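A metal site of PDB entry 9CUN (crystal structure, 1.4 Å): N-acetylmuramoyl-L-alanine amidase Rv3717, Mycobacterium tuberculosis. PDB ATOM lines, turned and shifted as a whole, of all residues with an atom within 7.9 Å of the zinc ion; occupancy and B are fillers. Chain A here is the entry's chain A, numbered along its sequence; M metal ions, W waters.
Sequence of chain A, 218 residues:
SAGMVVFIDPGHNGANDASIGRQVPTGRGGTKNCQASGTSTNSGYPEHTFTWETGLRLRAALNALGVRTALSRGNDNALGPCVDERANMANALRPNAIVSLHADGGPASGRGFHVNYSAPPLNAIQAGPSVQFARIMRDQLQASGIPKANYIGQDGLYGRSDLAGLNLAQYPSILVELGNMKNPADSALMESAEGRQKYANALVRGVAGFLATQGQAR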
ATOM      1  N   GLY A  11      13.313  18.281 -11.977  1.00  0.00           N
ATOM      2  CA  GLY A  11      14.124  19.331 -11.379  1.00  0.00           C
ATOM      3  C   GLY A  11      13.473  19.939 -10.143  1.00  0.00           C
ATOM      4  O   GLY A  11      12.248  20.036 -10.037  1.00  0.00           O
ATOM      5  N   HIS A  12      14.335  20.366  -9.224  1.00  0.00           N
ATOM      6  CA  HIS A  12      13.990  21.088  -8.003  1.00  0.00           C
ATOM      7  C   HIS A  12      13.418  20.173  -6.944  1.00  0.00           C
ATOM      8  O   HIS A  12      13.337  18.962  -7.141  1.00  0.00           O
ATOM      9  CB  HIS A  12      13.100  22.297  -8.320  1.00  0.00           C
ATOM     10  CG  HIS A  12      13.741  23.232  -9.268  1.00  0.00           C
ATOM     11  ND1 HIS A  12      14.740  24.116  -8.895  1.00  0.00           N
ATOM     12  CD2 HIS A  12      13.620  23.340 -10.606  1.00  0.00           C
ATOM     13  CE1 HIS A  12      15.160  24.766  -9.964  1.00  0.00           C
ATOM     14  NE2 HIS A  12      14.502  24.306 -11.015  1.00  0.00           N
ATOM     15  N   GLN A  35      20.736  23.824  -4.536  1.00  0.00           N
ATOM     16  CA  GLN A  35      19.513  23.779  -5.325  1.00  0.00           C
ATOM     17  C   GLN A  35      19.060  25.209  -5.554  1.00  0.00           C
ATOM     18  O   GLN A  35      19.266  26.066  -4.704  1.00  0.00           O
ATOM     19  CB  GLN A  35      18.375  23.058  -4.594  1.00  0.00           C
ATOM     20  CG  GLN A  35      18.247  21.577  -4.922  1.00  0.00           C
ATOM     21  CD  GLN A  35      17.960  21.307  -6.388  1.00  0.00           C
ATOM     22  OE1 GLN A  35      17.630  22.230  -7.155  1.00  0.00           O
ATOM     23  NE2 GLN A  35      18.107  20.064  -6.794  1.00  0.00           N
ATOM     24  N   ALA A  36      18.447  25.443  -6.705  1.00  0.00           N
ATOM     25  CA  ALA A  36      17.639  26.650  -6.892  1.00  0.00           C
ATOM     26  C   ALA A  36      16.205  26.324  -6.508  1.00  0.00           C
ATOM     27  O   ALA A  36      15.778  25.184  -6.616  1.00  0.00           O
ATOM     28  CB  ALA A  36      17.709  27.097  -8.356  1.00  0.00           C
ATOM     29  N   SER A  37      15.467  27.339  -6.037  1.00  0.00           N
ATOM     30  CA  SER A  37      14.071  27.107  -5.664  1.00  0.00           C
ATOM     31  C   SER A  37      13.226  26.720  -6.860  1.00  0.00           C
ATOM     32  O   SER A  37      12.288  25.922  -6.738  1.00  0.00           O
ATOM     33  CB  SER A  37      13.495  28.345  -4.990  1.00  0.00           C
ATOM     34  OG  SER A  37      13.449  29.439  -5.904  1.00  0.00           O
ATOM     35  N   GLY A  38      13.537  27.265  -8.035  1.00  0.00           N
ATOM     36  CA  GLY A  38      12.693  27.071  -9.192  1.00  0.00           C
ATOM     37  C   GLY A  38      11.706  28.213  -9.368  1.00  0.00           C
ATOM     38  O   GLY A  38      11.522  29.069  -8.495  1.00  0.00           O
ATOM     39  N   THR A  39      11.056  28.234 -10.527  1.00  0.00           N
ATOM     40  CA  THR A  39      10.163  29.328 -10.892  1.00  0.00           C
ATOM     41  C   THR A  39       8.702  28.879 -10.789  1.00  0.00           C
ATOM     42  O   THR A  39       8.397  27.874 -10.149  1.00  0.00           O
ATOM     43  CB  THR A  39      10.565  29.886 -12.269  1.00  0.00           C
ATOM     44  OG1 THR A  39       9.802  31.075 -12.549  1.00  0.00           O
ATOM     45  CG2 THR A  39      10.351  28.854 -13.373  1.00  0.00           C
ATOM     46  N   GLU A  47       7.313  25.302 -10.736  1.00  0.00           N
ATOM     47  CA  GLU A  47       8.204  24.479 -11.555  1.00  0.00           C
ATOM     48  C   GLU A  47       8.373  23.074 -10.966  1.00  0.00           C
ATOM     49  O   GLU A  47       8.303  22.081 -11.684  1.00  0.00           O
ATOM     50  CB  GLU A  47       9.553  25.168 -11.726  1.00  0.00           C
ATOM     51  CG  GLU A  47      10.491  24.380 -12.630  1.00  0.00           C
ATOM     52  CD  GLU A  47      11.860  25.010 -12.731  1.00  0.00           C
ATOM     53  OE1 GLU A  47      12.063  26.119 -12.177  1.00  0.00           O
ATOM     54  OE2 GLU A  47      12.747  24.404 -13.376  1.00  0.00           O
ATOM     55  N   HIS A  48       8.630  22.978  -9.657  1.00  0.00           N
ATOM     56  CA  HIS A  48       8.905  21.672  -9.085  1.00  0.00           C
ATOM     57  C   HIS A  48       7.719  20.728  -9.252  1.00  0.00           C
ATOM     58  O   HIS A  48       7.916  19.511  -9.384  1.00  0.00           O
ATOM     59  CB  HIS A  48       9.335  21.805  -7.621  1.00  0.00           C
ATOM     60  CG  HIS A  48       8.225  22.178  -6.676  1.00  0.00           C
ATOM     61  ND1 HIS A  48       7.348  21.252  -6.150  1.00  0.00           N
ATOM     62  CD2 HIS A  48       7.859  23.382  -6.156  1.00  0.00           C
ATOM     63  CE1 HIS A  48       6.497  21.861  -5.339  1.00  0.00           C
ATOM     64  NE2 HIS A  48       6.782  23.159  -5.329  1.00  0.00           N
ATOM     65  N   THR A  51       7.598  19.703 -13.111  1.00  0.00           N
ATOM     66  CA  THR A  51       8.600  18.713 -13.504  1.00  0.00           C
ATOM     67  C   THR A  51       8.274  17.357 -12.886  1.00  0.00           C
ATOM     68  O   THR A  51       8.491  16.312 -13.521  1.00  0.00           O
ATOM     69  CB  THR A  51      10.001  19.164 -13.086  1.00  0.00           C
ATOM     70  OG1 THR A  51      10.067  19.231 -11.650  1.00  0.00           O
ATOM     71  CG2 THR A  51      10.345  20.526 -13.699  1.00  0.00           C
ATOM     72  N   SER A 100      17.040  15.267 -17.239  1.00  0.00           N
ATOM     73  CA  SER A 100      16.548  16.189 -16.218  1.00  0.00           C
ATOM     74  C   SER A 100      15.506  17.096 -16.863  1.00  0.00           C
ATOM     75  O   SER A 100      15.643  17.494 -18.026  1.00  0.00           O
ATOM     76  CB  SER A 100      17.708  17.003 -15.650  1.00  0.00           C
ATOM     77  OG  SER A 100      17.253  17.966 -14.722  1.00  0.00           O
ATOM     78  N   LEU A 101      14.426  17.359 -16.116  1.00  0.00           N
ATOM     79  CA  LEU A 101      13.297  18.145 -16.596  1.00  0.00           C
ATOM     80  C   LEU A 101      13.191  19.432 -15.794  1.00  0.00           C
ATOM     81  O   LEU A 101      13.145  19.385 -14.549  1.00  0.00           O
ATOM     82  CB  LEU A 101      11.987  17.360 -16.451  1.00  0.00           C
ATOM     83  CG  LEU A 101      11.976  15.981 -17.094  1.00  0.00           C
ATOM     84  CD1 LEU A 101      10.588  15.386 -16.897  1.00  0.00           C
ATOM     85  CD2 LEU A 101      12.330  16.109 -18.573  1.00  0.00           C
ATOM     86  N   HIS A 102      13.094  20.556 -16.500  1.00  0.00           N
ATOM     87  CA  HIS A 102      13.008  21.877 -15.909  1.00  0.00           C
ATOM     88  C   HIS A 102      12.037  22.723 -16.722  1.00  0.00           C
ATOM     89  O   HIS A 102      11.617  22.349 -17.817  1.00  0.00           O
ATOM     90  CB  HIS A 102      14.370  22.569 -15.874  1.00  0.00           C
ATOM     91  CG  HIS A 102      15.259  22.083 -14.782  1.00  0.00           C
ATOM     92  ND1 HIS A 102      15.515  22.826 -13.653  1.00  0.00           N
ATOM     93  CD2 HIS A 102      15.943  20.920 -14.630  1.00  0.00           C
ATOM     94  CE1 HIS A 102      16.301  22.139 -12.835  1.00  0.00           C
ATOM     95  NE2 HIS A 102      16.580  20.991 -13.418  1.00  0.00           N
ATOM     96  N   ALA A 103      11.706  23.885 -16.160  1.00  0.00           N
ATOM     97  CA  ALA A 103      11.039  24.932 -16.926  1.00  0.00           C
ATOM     98  C   ALA A 103      11.647  26.262 -16.539  1.00  0.00           C
ATOM     99  O   ALA A 103      12.175  26.438 -15.439  1.00  0.00           O
ATOM    100  CB  ALA A 103       9.528  24.936 -16.682  1.00  0.00           C
ATOM    101  N   ASP A 104      11.570  27.212 -17.447  1.00  0.00           N
ATOM    102  CA  ASP A 104      12.343  28.433 -17.341  1.00  0.00           C
ATOM    103  C   ASP A 104      11.484  29.586 -16.872  1.00  0.00           C
ATOM    104  O   ASP A 104      10.260  29.581 -17.020  1.00  0.00           O
ATOM    105  CB  ASP A 104      12.964  28.742 -18.705  1.00  0.00           C
ATOM    106  CG  ASP A 104      14.093  29.734 -18.619  1.00  0.00           C
ATOM    107  OD1 ASP A 104      14.741  29.869 -17.550  1.00  0.00           O
ATOM    108  OD2 ASP A 104      14.355  30.391 -19.644  1.00  0.00           O
ATOM    109  N   GLY A 105      12.140  30.578 -16.278  1.00  0.00           N
ATOM    110  CA  GLY A 105      11.476  31.835 -15.985  1.00  0.00           C
ATOM    111  C   GLY A 105      12.087  32.971 -16.763  1.00  0.00           C
ATOM    112  O   GLY A 105      13.050  33.604 -16.289  1.00  0.00           O
ATOM    113  N   LEU A 175      19.618  18.082 -20.056  1.00  0.00           N
ATOM    114  CA  LEU A 175      18.660  18.791 -19.217  1.00  0.00           C
ATOM    115  C   LEU A 175      17.724  19.574 -20.114  1.00  0.00           C
ATOM    116  O   LEU A 175      18.168  20.443 -20.884  1.00  0.00           O
ATOM    117  CB  LEU A 175      19.385  19.686 -18.208  1.00  0.00           C
ATOM    118  CG  LEU A 175      18.489  20.415 -17.199  1.00  0.00           C
ATOM    119  CD1 LEU A 175      19.266  20.666 -15.883  1.00  0.00           C
ATOM    120  CD2 LEU A 175      17.894  21.707 -17.782  1.00  0.00           C
ATOM    121  N   VAL A 176      16.437  19.251 -20.073  1.00  0.00           N
ATOM    122  CA  VAL A 176      15.460  19.835 -20.977  1.00  0.00           C
ATOM    123  C   VAL A 176      14.685  20.932 -20.258  1.00  0.00           C
ATOM    124  O   VAL A 176      13.965  20.656 -19.288  1.00  0.00           O
ATOM    125  CB  VAL A 176      14.480  18.776 -21.516  1.00  0.00           C
ATOM    126  CG1 VAL A 176      13.499  19.413 -22.502  1.00  0.00           C
ATOM    127  CG2 VAL A 176      15.247  17.618 -22.179  1.00  0.00           C
ATOM    128  N   GLU A 177      14.838  22.165 -20.715  1.00  0.00           N
ATOM    129  CA  GLU A 177      13.964  23.267 -20.323  1.00  0.00           C
ATOM    130  C   GLU A 177      12.764  23.252 -21.256  1.00  0.00           C
ATOM    131  O   GLU A 177      12.895  23.560 -22.447  1.00  0.00           O
ATOM    132  CB  GLU A 177      14.726  24.588 -20.393  1.00  0.00           C
ATOM    133  CG  GLU A 177      15.824  24.730 -19.333  1.00  0.00           C
ATOM    134  CD  GLU A 177      15.265  25.141 -17.976  1.00  0.00           C
ATOM    135  OE1 GLU A 177      14.031  25.305 -17.838  1.00  0.00           O
ATOM    136  OE2 GLU A 177      16.083  25.314 -17.033  1.00  0.00           O
ATOM    137  N   MET A 181       7.740  29.384 -18.097  1.00  0.00           N
ATOM    138  CA  MET A 181       6.546  29.377 -17.263  1.00  0.00           C
ATOM    139  C   MET A 181       5.851  30.717 -17.246  1.00  0.00           C
ATOM    140  O   MET A 181       4.667  30.776 -16.910  1.00  0.00           O
ATOM    141  CB  MET A 181       6.916  29.011 -15.819  1.00  0.00           C
ATOM    142  CG  MET A 181       7.602  27.651 -15.678  1.00  0.00           C
ATOM    143  SD  MET A 181       7.394  26.900 -14.046  1.00  0.00           S
ATOM    144  CE  MET A 181       5.916  25.951 -14.253  1.00  0.00           C
HETATM  145 ZN    ZN M   1      14.764  24.776 -13.061  1.00  0.00          ZN
HETATM  146  O   HOH W   1      14.394  26.939 -12.403  1.00  0.00           O
HETATM  147  O   HOH W   2      14.798  25.821 -14.797  1.00  0.00           O
HETATM  148  O   HOH W   3      16.798  25.566 -12.639  1.00  0.00           O
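OE2 of Glu 47 lies close to N of Ala 103 (3.0 Å). N of Glu 47 is in hydrogen-bond range of O of Thr 39 (2.9 Å). The side-chain hydroxyl (OG1) of Thr 51 sits close to the backbone carbonyl oxygen (O) of Glu 47. The backbone NH (N) of Glu 47 sits close to the side-chain sulfur (SD) of Met 181, at 3.7 Å. A ring nitrogen (ND1) of His 12 lies within hydrogen-bond range of the backbone NH (N) of Gly 38 (3.5 Å). ND1 of His 12 sits at hydrogen-bond distance from O of Ala 36 (2.7 Å). A ring nitrogen (NE2) of His 102 sits close to the side-chain hydroxyl of Ser 100 (3.4 Å). The backbone carbonyl oxygen of Val 176 sits at hydrogen-bond distance from the backbone NH of His 102 (2.9 Å).
Water W2 bridges the side-chain carboxylate (OE2) of Glu 177 (2.6 Å) and the backbone carbonyl oxygen (O) of Ala 103 (2.8 Å).
The zinc ion is bound by water W2 (2.0 Å), the side-chain carboxylate of Glu 47 (2.1 Å), a ring nitrogen (NE2) of His 12 (2.1 Å), a ring nitrogen (ND1) of His 102 (2.2 Å), water W3 (2.2 Å) and water W1 (2.3 Å). The zinc ion has six donor atoms within binding distance.
O of Ala 103 touches the zinc ion (3.9 Å). Of the 20 residues printed, 4 come within 4 Å of the zinc ion. The nearest printed residue that does not touch the zinc ion is Glu 177 (4.2 Å).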
